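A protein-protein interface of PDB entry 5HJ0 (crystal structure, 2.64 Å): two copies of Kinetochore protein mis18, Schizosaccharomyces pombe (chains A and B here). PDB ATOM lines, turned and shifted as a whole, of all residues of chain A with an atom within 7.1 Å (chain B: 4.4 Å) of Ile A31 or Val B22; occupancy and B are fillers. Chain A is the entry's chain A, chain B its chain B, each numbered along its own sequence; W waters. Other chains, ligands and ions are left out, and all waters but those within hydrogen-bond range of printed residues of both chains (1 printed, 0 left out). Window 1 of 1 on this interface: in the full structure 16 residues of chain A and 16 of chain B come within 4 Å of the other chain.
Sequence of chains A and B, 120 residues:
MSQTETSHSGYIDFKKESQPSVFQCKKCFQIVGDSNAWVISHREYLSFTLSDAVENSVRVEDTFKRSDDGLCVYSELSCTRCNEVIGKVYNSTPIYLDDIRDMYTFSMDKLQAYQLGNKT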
ATOM      1  N   PRO A  20      13.778 -18.455 -19.778  1.00  0.00           N
ATOM      2  CA  PRO A  20      13.489 -17.138 -19.217  1.00  0.00           C
ATOM      3  C   PRO A  20      14.733 -16.373 -18.809  1.00  0.00           C
ATOM      4  O   PRO A  20      15.773 -16.977 -18.524  1.00  0.00           O
ATOM      5  CB  PRO A  20      12.660 -17.453 -17.962  1.00  0.00           C
ATOM      6  CG  PRO A  20      12.533 -18.935 -17.876  1.00  0.00           C
ATOM      7  CD  PRO A  20      13.575 -19.517 -18.775  1.00  0.00           C
ATOM      8  N   SER A  21      14.609 -15.050 -18.773  1.00  0.00           N
ATOM      9  CA  SER A  21      15.672 -14.159 -18.325  1.00  0.00           C
ATOM     10  C   SER A  21      15.297 -13.439 -17.032  1.00  0.00           C
ATOM     11  O   SER A  21      14.117 -13.289 -16.709  1.00  0.00           O
ATOM     12  CB  SER A  21      16.022 -13.140 -19.413  1.00  0.00           C
ATOM     13  OG  SER A  21      16.674 -13.760 -20.506  1.00  0.00           O
ATOM     14  N   VAL A  22      16.321 -13.002 -16.305  1.00  0.00           N
ATOM     15  CA  VAL A  22      16.184 -12.265 -15.058  1.00  0.00           C
ATOM     16  C   VAL A  22      16.830 -10.897 -15.275  1.00  0.00           C
ATOM     17  O   VAL A  22      17.835 -10.793 -15.984  1.00  0.00           O
ATOM     18  CB  VAL A  22      16.833 -13.069 -13.913  1.00  0.00           C
ATOM     19  CG1 VAL A  22      17.488 -12.188 -12.864  1.00  0.00           C
ATOM     20  CG2 VAL A  22      15.806 -13.982 -13.280  1.00  0.00           C
ATOM     21  N   PHE A  23      16.253  -9.855 -14.681  1.00  0.00           N
ATOM     22  CA  PHE A  23      16.719  -8.495 -14.926  1.00  0.00           C
ATOM     23  C   PHE A  23      17.281  -7.867 -13.682  1.00  0.00           C
ATOM     24  O   PHE A  23      16.691  -7.946 -12.601  1.00  0.00           O
ATOM     25  CB  PHE A  23      15.597  -7.629 -15.499  1.00  0.00           C
ATOM     26  CG  PHE A  23      15.005  -8.177 -16.760  1.00  0.00           C
ATOM     27  CD1 PHE A  23      15.721  -8.117 -17.969  1.00  0.00           C
ATOM     28  CD2 PHE A  23      13.751  -8.773 -16.743  1.00  0.00           C
ATOM     29  CE1 PHE A  23      15.192  -8.645 -19.140  1.00  0.00           C
ATOM     30  CE2 PHE A  23      13.208  -9.283 -17.914  1.00  0.00           C
ATOM     31  CZ  PHE A  23      13.926  -9.224 -19.110  1.00  0.00           C
ATOM     32  N   GLN A  24      18.425  -7.229 -13.863  1.00  0.00           N
ATOM     33  CA  GLN A  24      19.220  -6.725 -12.763  1.00  0.00           C
ATOM     34  C   GLN A  24      19.545  -5.280 -12.995  1.00  0.00           C
ATOM     35  O   GLN A  24      19.838  -4.873 -14.127  1.00  0.00           O
ATOM     36  CB  GLN A  24      20.565  -7.451 -12.700  1.00  0.00           C
ATOM     37  CG  GLN A  24      20.552  -8.866 -12.174  1.00  0.00           C
ATOM     38  CD  GLN A  24      21.935  -9.491 -12.275  1.00  0.00           C
ATOM     39  OE1 GLN A  24      22.445  -9.712 -13.372  1.00  0.00           O
ATOM     40  NE2 GLN A  24      22.548  -9.776 -11.129  1.00  0.00           N
ATOM     41  N   CYS A  25      19.543  -4.513 -11.915  1.00  0.00           N
ATOM     42  CA  CYS A  25      20.194  -3.225 -11.937  1.00  0.00           C
ATOM     43  C   CYS A  25      21.667  -3.422 -12.351  1.00  0.00           C
ATOM     44  O   CYS A  25      22.339  -4.348 -11.883  1.00  0.00           O
ATOM     45  CB  CYS A  25      20.069  -2.561 -10.576  1.00  0.00           C
ATOM     46  SG  CYS A  25      21.062  -1.083 -10.418  1.00  0.00           S
ATOM     47  N   CYS A  28      24.572  -1.801  -8.785  1.00  0.00           N
ATOM     48  CA  CYS A  28      24.483  -2.822  -7.758  1.00  0.00           C
ATOM     49  C   CYS A  28      23.854  -3.940  -8.552  1.00  0.00           C
ATOM     50  O   CYS A  28      23.390  -3.676  -9.669  1.00  0.00           O
ATOM     51  CB  CYS A  28      23.527  -2.326  -6.677  1.00  0.00           C
ATOM     52  SG  CYS A  28      21.757  -2.506  -7.061  1.00  0.00           S
ATOM     53  N   PHE A  29      23.794  -5.170  -8.070  1.00  0.00           N
ATOM     54  CA  PHE A  29      23.271  -6.147  -9.040  1.00  0.00           C
ATOM     55  C   PHE A  29      21.894  -6.729  -8.734  1.00  0.00           C
ATOM     56  O   PHE A  29      21.575  -7.872  -9.099  1.00  0.00           O
ATOM     57  CB  PHE A  29      24.336  -7.165  -9.430  1.00  0.00           C
ATOM     58  CG  PHE A  29      25.448  -6.557 -10.229  1.00  0.00           C
ATOM     59  CD1 PHE A  29      26.598  -6.063  -9.595  1.00  0.00           C
ATOM     60  CD2 PHE A  29      25.341  -6.442 -11.617  1.00  0.00           C
ATOM     61  CE1 PHE A  29      27.626  -5.483 -10.336  1.00  0.00           C
ATOM     62  CE2 PHE A  29      26.366  -5.862 -12.363  1.00  0.00           C
ATOM     63  CZ  PHE A  29      27.512  -5.382 -11.722  1.00  0.00           C
ATOM     64  N   GLN A  30      21.073  -5.892  -8.094  1.00  0.00           N
ATOM     65  CA  GLN A  30      19.808  -6.306  -7.532  1.00  0.00           C
ATOM     66  C   GLN A  30      18.839  -6.685  -8.619  1.00  0.00           C
ATOM     67  O   GLN A  30      18.681  -5.952  -9.597  1.00  0.00           O
ATOM     68  CB  GLN A  30      19.230  -5.201  -6.675  1.00  0.00           C
ATOM     69  CG  GLN A  30      17.993  -5.598  -5.895  1.00  0.00           C
ATOM     70  CD  GLN A  30      17.730  -4.638  -4.772  1.00  0.00           C
ATOM     71  OE1 GLN A  30      17.333  -3.492  -5.004  1.00  0.00           O
ATOM     72  NE2 GLN A  30      17.977  -5.078  -3.548  1.00  0.00           N
ATOM     73  N   ILE A  31      18.235  -7.859  -8.439  1.00  0.00           N
ATOM     74  CA  ILE A  31      17.228  -8.410  -9.349  1.00  0.00           C
ATOM     75  C   ILE A  31      15.914  -7.634  -9.169  1.00  0.00           C
ATOM     76  O   ILE A  31      15.348  -7.626  -8.077  1.00  0.00           O
ATOM     77  CB  ILE A  31      17.049  -9.939  -9.125  1.00  0.00           C
ATOM     78  CG1 ILE A  31      18.290 -10.680  -9.631  1.00  0.00           C
ATOM     79  CG2 ILE A  31      15.787 -10.466  -9.801  1.00  0.00           C
ATOM     80  CD1 ILE A  31      18.341 -12.165  -9.304  1.00  0.00           C
ATOM     81  N   VAL A  32      15.460  -6.987 -10.241  1.00  0.00           N
ATOM     82  CA  VAL A  32      14.265  -6.117 -10.195  1.00  0.00           C
ATOM     83  C   VAL A  32      12.993  -6.875 -10.569  1.00  0.00           C
ATOM     84  O   VAL A  32      11.889  -6.511 -10.165  1.00  0.00           O
ATOM     85  CB  VAL A  32      14.416  -4.856 -11.066  1.00  0.00           C
ATOM     86  CG1 VAL A  32      15.581  -4.022 -10.571  1.00  0.00           C
ATOM     87  CG2 VAL A  32      14.599  -5.218 -12.529  1.00  0.00           C
ATOM     88  N   GLY A  33      13.182  -7.946 -11.328  1.00  0.00           N
ATOM     89  CA  GLY A  33      12.112  -8.810 -11.785  1.00  0.00           C
ATOM     90  C   GLY A  33      12.601  -9.633 -12.956  1.00  0.00           C
ATOM     91  O   GLY A  33      13.735  -9.477 -13.423  1.00  0.00           O
ATOM     92  N   ASP A  34      11.741 -10.508 -13.444  1.00  0.00           N
ATOM     93  CA  ASP A  34      12.093 -11.365 -14.558  1.00  0.00           C
ATOM     94  C   ASP A  34      11.138 -11.203 -15.732  1.00  0.00           C
ATOM     95  O   ASP A  34      10.019 -10.696 -15.588  1.00  0.00           O
ATOM     96  CB  ASP A  34      12.142 -12.829 -14.100  1.00  0.00           C
ATOM     97  CG  ASP A  34      10.891 -13.250 -13.338  1.00  0.00           C
ATOM     98  OD1 ASP A  34       9.797 -13.344 -13.946  1.00  0.00           O
ATOM     99  OD2 ASP A  34      10.996 -13.496 -12.117  1.00  0.00           O
ATOM    100  N   ALA A  53       7.199  -6.802 -10.607  1.00  0.00           N
ATOM    101  CA  ALA A  53       8.564  -6.515 -10.213  1.00  0.00           C
ATOM    102  C   ALA A  53       8.761  -6.963  -8.773  1.00  0.00           C
ATOM    103  O   ALA A  53       7.790  -7.163  -8.045  1.00  0.00           O
ATOM    104  CB  ALA A  53       8.853  -5.034 -10.352  1.00  0.00           C
ATOM    105  N   VAL A  54      10.015  -7.128  -8.367  1.00  0.00           N
ATOM    106  CA  VAL A  54      10.314  -7.493  -7.001  1.00  0.00           C
ATOM    107  C   VAL A  54       9.990  -6.288  -6.126  1.00  0.00           C
ATOM    108  O   VAL A  54      10.553  -5.207  -6.315  1.00  0.00           O
ATOM    109  CB  VAL A  54      11.785  -7.946  -6.820  1.00  0.00           C
ATOM    110  CG1 VAL A  54      11.987  -8.489  -5.418  1.00  0.00           C
ATOM    111  CG2 VAL A  54      12.159  -9.003  -7.846  1.00  0.00           C
ATOM    112  N   GLU A  55       9.079  -6.483  -5.177  1.00  0.00           N
ATOM    113  CA  GLU A  55       8.574  -5.383  -4.352  1.00  0.00           C
ATOM    114  C   GLU A  55       9.676  -4.600  -3.632  1.00  0.00           C
ATOM    115  O   GLU A  55       9.714  -3.383  -3.761  1.00  0.00           O
ATOM    116  CB  GLU A  55       7.512  -5.863  -3.364  1.00  0.00           C
ATOM    117  CG  GLU A  55       6.458  -4.811  -3.045  1.00  0.00           C
ATOM    118  CD  GLU A  55       5.224  -4.895  -3.938  1.00  0.00           C
ATOM    119  OE1 GLU A  55       4.103  -4.800  -3.387  1.00  0.00           O
ATOM    120  OE2 GLU A  55       5.354  -5.056  -5.178  1.00  0.00           O
ATOM    121  N   ASN A  56      10.579  -5.290  -2.923  1.00  0.00           N
ATOM    122  CA  ASN A  56      11.655  -4.619  -2.167  1.00  0.00           C
ATOM    123  C   ASN A  56      12.759  -4.060  -3.038  1.00  0.00           C
ATOM    124  O   ASN A  56      13.575  -3.294  -2.561  1.00  0.00           O
ATOM    125  CB  ASN A  56      12.329  -5.546  -1.142  1.00  0.00           C
ATOM    126  CG  ASN A  56      11.346  -6.339  -0.297  1.00  0.00           C
ATOM    127  OD1 ASN A  56      10.123  -6.137  -0.344  1.00  0.00           O
ATOM    128  ND2 ASN A  56      11.887  -7.266   0.495  1.00  0.00           N
ATOM    129  N   SER A  57      12.823  -4.458  -4.300  1.00  0.00           N
ATOM    130  CA  SER A  57      13.967  -4.074  -5.126  1.00  0.00           C
ATOM    131  C   SER A  57      13.772  -2.740  -5.816  1.00  0.00           C
ATOM    132  O   SER A  57      14.721  -2.125  -6.285  1.00  0.00           O
ATOM    133  CB  SER A  57      14.271  -5.171  -6.129  1.00  0.00           C
ATOM    134  OG  SER A  57      14.641  -6.335  -5.416  1.00  0.00           O
ATOM    135  N   VAL A  58      12.531  -2.280  -5.800  1.00  0.00           N
ATOM    136  CA  VAL A  58      12.069  -1.211  -6.646  1.00  0.00           C
ATOM    137  C   VAL A  58      11.215  -0.251  -5.813  1.00  0.00           C
ATOM    138  O   VAL A  58      10.431  -0.687  -4.977  1.00  0.00           O
ATOM    139  CB  VAL A  58      11.341  -1.867  -7.831  1.00  0.00           C
ATOM    140  CG1 VAL A  58       9.919  -1.363  -8.024  1.00  0.00           C
ATOM    141  CG2 VAL A  58      12.201  -1.781  -9.078  1.00  0.00           C
ATOM    142  N   TYR A 114      20.091 -11.627 -17.399  1.00  0.00           N
ATOM    143  CA  TYR A 114      20.739 -12.918 -17.290  1.00  0.00           C
ATOM    144  C   TYR A 114      19.765 -13.976 -17.756  1.00  0.00           C
ATOM    145  O   TYR A 114      18.679 -14.119 -17.181  1.00  0.00           O
ATOM    146  CB  TYR A 114      21.178 -13.205 -15.852  1.00  0.00           C
ATOM    147  CG  TYR A 114      21.619 -14.638 -15.618  1.00  0.00           C
ATOM    148  CD1 TYR A 114      22.860 -15.085 -16.079  1.00  0.00           C
ATOM    149  CD2 TYR A 114      20.791 -15.552 -14.939  1.00  0.00           C
ATOM    150  CE1 TYR A 114      23.272 -16.394 -15.873  1.00  0.00           C
ATOM    151  CE2 TYR A 114      21.192 -16.869 -14.734  1.00  0.00           C
ATOM    152  CZ  TYR A 114      22.440 -17.279 -15.199  1.00  0.00           C
ATOM    153  OH  TYR A 114      22.882 -18.564 -14.999  1.00  0.00           O
ATOM    154  N   GLN A 115      20.158 -14.711 -18.796  1.00  0.00           N
ATOM    155  CA  GLN A 115      19.375 -15.836 -19.282  1.00  0.00           C
ATOM    156  C   GLN A 115      19.877 -17.125 -18.633  1.00  0.00           C
ATOM    157  O   GLN A 115      21.086 -17.365 -18.581  1.00  0.00           O
ATOM    158  CB  GLN A 115      19.452 -15.922 -20.803  1.00  0.00           C
ATOM    159  CG  GLN A 115      18.560 -17.003 -21.401  1.00  0.00           C
ATOM    160  CD  GLN A 115      18.400 -16.885 -22.902  1.00  0.00           C
ATOM    161  OE1 GLN A 115      19.314 -16.460 -23.615  1.00  0.00           O
ATOM    162  NE2 GLN A 115      17.231 -17.275 -23.398  1.00  0.00           N
ATOM    163  N   LEU A 116      18.944 -17.943 -18.145  1.00  0.00           N
ATOM    164  CA  LEU A 116      19.276 -19.217 -17.506  1.00  0.00           C
ATOM    165  C   LEU A 116      19.809 -20.235 -18.519  1.00  0.00           C
ATOM    166  O   LEU A 116      19.466 -20.183 -19.706  1.00  0.00           O
ATOM    167  CB  LEU A 116      18.084 -19.832 -16.751  1.00  0.00           C
ATOM    168  CG  LEU A 116      17.004 -19.160 -15.900  1.00  0.00           C
ATOM    169  CD1 LEU A 116      16.714 -20.062 -14.720  1.00  0.00           C
ATOM    170  CD2 LEU A 116      17.317 -17.758 -15.399  1.00  0.00           C
ATOM    171  N   SER B  21      15.016 -21.281 -10.066  1.00  0.00           N
ATOM    172  CA  SER B  21      15.647 -20.238  -9.264  1.00  0.00           C
ATOM    173  C   SER B  21      16.981 -19.781  -9.880  1.00  0.00           C
ATOM    174  O   SER B  21      17.522 -20.427 -10.781  1.00  0.00           O
ATOM    175  CB  SER B  21      15.831 -20.691  -7.813  1.00  0.00           C
ATOM    176  OG  SER B  21      14.584 -20.809  -7.148  1.00  0.00           O
ATOM    177  N   VAL B  22      17.470 -18.641  -9.393  1.00  0.00           N
ATOM    178  CA  VAL B  22      18.725 -18.014  -9.799  1.00  0.00           C
ATOM    179  C   VAL B  22      19.449 -17.734  -8.491  1.00  0.00           C
ATOM    180  O   VAL B  22      18.813 -17.345  -7.500  1.00  0.00           O
ATOM    181  CB  VAL B  22      18.447 -16.712 -10.592  1.00  0.00           C
ATOM    182  CG1 VAL B  22      19.582 -15.705 -10.493  1.00  0.00           C
ATOM    183  CG2 VAL B  22      18.177 -17.033 -12.045  1.00  0.00           C
ATOM    184  N   PHE B  23      20.764 -17.950  -8.479  1.00  0.00           N
ATOM    185  CA  PHE B  23      21.534 -17.840  -7.241  1.00  0.00           C
ATOM    186  C   PHE B  23      22.566 -16.747  -7.328  1.00  0.00           C
ATOM    187  O   PHE B  23      23.278 -16.637  -8.320  1.00  0.00           O
ATOM    188  CB  PHE B  23      22.205 -19.159  -6.885  1.00  0.00           C
ATOM    189  CG  PHE B  23      21.282 -20.337  -6.899  1.00  0.00           C
ATOM    190  CD1 PHE B  23      20.416 -20.577  -5.832  1.00  0.00           C
ATOM    191  CD2 PHE B  23      21.288 -21.223  -7.980  1.00  0.00           C
ATOM    192  CE1 PHE B  23      19.566 -21.673  -5.846  1.00  0.00           C
ATOM    193  CE2 PHE B  23      20.442 -22.327  -8.002  1.00  0.00           C
ATOM    194  CZ  PHE B  23      19.580 -22.550  -6.930  1.00  0.00           C
ATOM    195  N   GLN B  24      22.625 -15.945  -6.272  1.00  0.00           N
ATOM    196  CA  GLN B  24      23.491 -14.785  -6.210  1.00  0.00           C
ATOM    197  C   GLN B  24      24.294 -14.799  -4.940  1.00  0.00           C
ATOM    198  O   GLN B  24      23.815 -15.245  -3.886  1.00  0.00           O
ATOM    199  CB  GLN B  24      22.679 -13.501  -6.144  1.00  0.00           C
ATOM    200  CG  GLN B  24      21.725 -13.216  -7.274  1.00  0.00           C
ATOM    201  CD  GLN B  24      20.858 -12.029  -6.927  1.00  0.00           C
ATOM    202  OE1 GLN B  24      21.019 -10.951  -7.492  1.00  0.00           O
ATOM    203  NE2 GLN B  24      19.950 -12.213  -5.967  1.00  0.00           N
ATOM    204  N   ILE B  31      25.179 -12.914  -9.907  1.00  0.00           N
ATOM    205  CA  ILE B  31      24.608 -14.209 -10.282  1.00  0.00           C
ATOM    206  C   ILE B  31      25.719 -15.241 -10.555  1.00  0.00           C
ATOM    207  O   ILE B  31      26.506 -15.104 -11.493  1.00  0.00           O
ATOM    208  CB  ILE B  31      23.621 -14.081 -11.471  1.00  0.00           C
ATOM    209  CG1 ILE B  31      22.406 -13.243 -11.047  1.00  0.00           C
ATOM    210  CG2 ILE B  31      23.176 -15.453 -11.956  1.00  0.00           C
ATOM    211  CD1 ILE B  31      21.436 -12.897 -12.162  1.00  0.00           C
ATOM    212  N   GLY B  33      25.025 -18.612 -10.786  1.00  0.00           N
ATOM    213  CA  GLY B  33      24.424 -19.689 -11.554  1.00  0.00           C
ATOM    214  C   GLY B  33      22.962 -19.857 -11.216  1.00  0.00           C
ATOM    215  O   GLY B  33      22.483 -19.395 -10.185  1.00  0.00           O
ATOM    216  N   ASP B  34      22.253 -20.525 -12.110  1.00  0.00           N
ATOM    217  CA  ASP B  34      20.847 -20.854 -11.906  1.00  0.00           C
ATOM    218  C   ASP B  34      20.662 -22.338 -11.620  1.00  0.00           C
ATOM    219  O   ASP B  34      21.560 -23.149 -11.876  1.00  0.00           O
ATOM    220  CB  ASP B  34      20.026 -20.448 -13.135  1.00  0.00           C
ATOM    221  CG  ASP B  34      20.613 -20.969 -14.431  1.00  0.00           C
ATOM    222  OD1 ASP B  34      20.549 -22.181 -14.678  1.00  0.00           O
ATOM    223  OD2 ASP B  34      21.147 -20.173 -15.219  1.00  0.00           O
ATOM    224  N   GLN B 112      21.997 -16.309  -1.991  1.00  0.00           N
ATOM    225  CA  GLN B 112      20.561 -16.134  -1.940  1.00  0.00           C
ATOM    226  C   GLN B 112      19.910 -16.517  -3.247  1.00  0.00           C
ATOM    227  O   GLN B 112      20.482 -16.328  -4.326  1.00  0.00           O
ATOM    228  CB  GLN B 112      20.169 -14.744  -1.452  1.00  0.00           C
ATOM    229  CG  GLN B 112      20.256 -13.618  -2.459  1.00  0.00           C
ATOM    230  CD  GLN B 112      19.640 -12.366  -1.885  1.00  0.00           C
ATOM    231  OE1 GLN B 112      20.024 -11.916  -0.799  1.00  0.00           O
ATOM    232  NE2 GLN B 112      18.659 -11.803  -2.593  1.00  0.00           N
ATOM    233  N   ALA B 113      18.721 -17.096  -3.118  1.00  0.00           N
ATOM    234  CA  ALA B 113      17.955 -17.579  -4.248  1.00  0.00           C
ATOM    235  C   ALA B 113      16.855 -16.583  -4.649  1.00  0.00           C
ATOM    236  O   ALA B 113      16.264 -15.894  -3.805  1.00  0.00           O
ATOM    237  CB  ALA B 113      17.360 -18.935  -3.924  1.00  0.00           C
ATOM    238  N   TYR B 114      16.622 -16.498  -5.952  1.00  0.00           N
ATOM    239  CA  TYR B 114      15.479 -15.805  -6.498  1.00  0.00           C
ATOM    240  C   TYR B 114      14.747 -16.789  -7.391  1.00  0.00           C
ATOM    241  O   TYR B 114      15.289 -17.197  -8.428  1.00  0.00           O
ATOM    242  CB  TYR B 114      15.914 -14.561  -7.293  1.00  0.00           C
ATOM    243  CG  TYR B 114      14.781 -13.899  -8.045  1.00  0.00           C
ATOM    244  CD1 TYR B 114      13.882 -13.053  -7.386  1.00  0.00           C
ATOM    245  CD2 TYR B 114      14.592 -14.134  -9.415  1.00  0.00           C
ATOM    246  CE1 TYR B 114      12.831 -12.463  -8.071  1.00  0.00           C
ATOM    247  CE2 TYR B 114      13.544 -13.545 -10.108  1.00  0.00           C
ATOM    248  CZ  TYR B 114      12.672 -12.710  -9.429  1.00  0.00           C
ATOM    249  OH  TYR B 114      11.639 -12.118 -10.103  1.00  0.00           O
ATOM    250  N   LEU B 116      11.820 -17.447 -10.034  1.00  0.00           N
ATOM    251  CA  LEU B 116      11.114 -16.663 -11.049  1.00  0.00           C
ATOM    252  C   LEU B 116       9.610 -16.757 -10.833  1.00  0.00           C
ATOM    253  O   LEU B 116       9.112 -17.760 -10.308  1.00  0.00           O
ATOM    254  CB  LEU B 116      11.467 -17.106 -12.474  1.00  0.00           C
ATOM    255  CG  LEU B 116      12.883 -17.297 -13.039  1.00  0.00           C
ATOM    256  CD1 LEU B 116      12.924 -16.590 -14.380  1.00  0.00           C
ATOM    257  CD2 LEU B 116      14.030 -16.800 -12.170  1.00  0.00           C
HETATM  258  O   HOH W   1      25.613 -10.338 -12.036  1.00  0.00           O
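OD2 of Asp A34 sits at hydrogen-bond distance from OH of Tyr B114, at 2.5 Å. The side-chain hydroxyl (OH) of Tyr A114 lies close to the side-chain carboxylate (OD2) of Asp B34 (2.4 Å).
The backbone NH (N) of Val A22 is in hydrogen-bond range of the backbone carbonyl oxygen (O) of Tyr A114. The backbone carbonyl oxygen of Gly A33 lies within hydrogen-bond range of the backbone NH of Phe A23. The side-chain amide nitrogen (NE2) of Gln A24 sits at hydrogen-bond distance from the backbone carbonyl oxygen (O) of Phe A29, 2.9 Å away. O of Val A32 is in hydrogen-bond range of N of Val A54. The backbone NH (N) of Phe B23 lies within hydrogen-bond range of the backbone carbonyl oxygen (O) of Gly B33. The backbone NH of Gln B112 lies within hydrogen-bond range of the backbone carbonyl oxygen of Gln B24.
Among the printed residues, pairs that only touch across the chains: Leu A116 with Asp B34 (3.1 Å), Asp A34 with Leu B116 (3.3 Å), Gln A24 with Ile B31 (3.4 Å), Ile A31 with Gln B24 (3.5 Å), Val A22 with Leu B116 (3.5 Å), Phe A29 with Gln B24 (3.5 Å), Val A54 with Tyr B114 (3.5 Å), Leu A116 with Val B22 (3.5 Å), Pro A20 with Leu B116 (3.7 Å), Tyr A114 with Ile B31 (3.7 Å), Gly A33 with Tyr B114 (3.7 Å), Ile A31 with Tyr B114 (3.8 Å), Val A22 with Tyr B114 (3.9 Å), Ile A31 with Val B22 (3.9 Å) and Tyr A114 with Gly B33 (3.9 Å).
Ile A31 touches three residues of chain B. Of chain A, only Ile A31 (3.9 Å) and Leu A116 (3.5 Å) come within 4 Å of Val B22. Of the printed residues of chain B, Pro A20 touches Leu B116. Of the printed residues of chain B, Val A54 touches Tyr B114 (3.5 Å). Printed residues of chain A within 4 Å of Gly B33: Tyr A114 (3.9 Å). Of the printed residues of chain A, Tyr B114 touches Val A22, Ile A31, Gly A33, Asp A34 and Val A54. Val A58 touches none of the printed residues of chain B. Gln B112 touches none of the printed residues of chain A. The nearest printed residue of chain A that does not touch Val B22 is Tyr A114 (4.04 Å).
Hydrophobic or aromatic side chains of chain B within 4 Å of the printed part of chain A: Val B22, Ile B31, Tyr B114 and Leu B116. Along chain B the printed residues that touch a printed residue of chain A span positions 22 to 116. Hydrophobic or aromatic side chains of chain A within 4 Å of the printed part of chain B: Pro A20, Val A22, Ile A31, Val A54, Tyr A114 and Leu A116. Among the printed residues, no Asp or Glu carboxylate lies within 4 Å of a Lys or Arg side-chain nitrogen of the other chain.
Val A22 touches Tyr B114, but with the chains exchanged Tyr A114 does not touch Val B22 (4.04 Å). Ile A31 touches Val B22, but with the chains exchanged Val A22 does not touch Ile B31 (4.1 Å). Ile A31 touches Tyr B114, and with the chains exchanged Tyr A114 touches Ile B31. Asp A34 touches Leu B116, and with the chains exchanged Leu A116 touches Asp B34. Positions printed for both chains: 21, 22, 23, 24, 31, 33, 34, 114 and 116. Of the 17 pairs that touch across the chains among the printed residues, 12 have their exchanged pair printed and touching as well.
Water W1 bridges the side-chain amide nitrogen (NE2) of Gln A24 (3.2 Å) and the backbone NH (N) of Ile B31 (3.4 Å).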
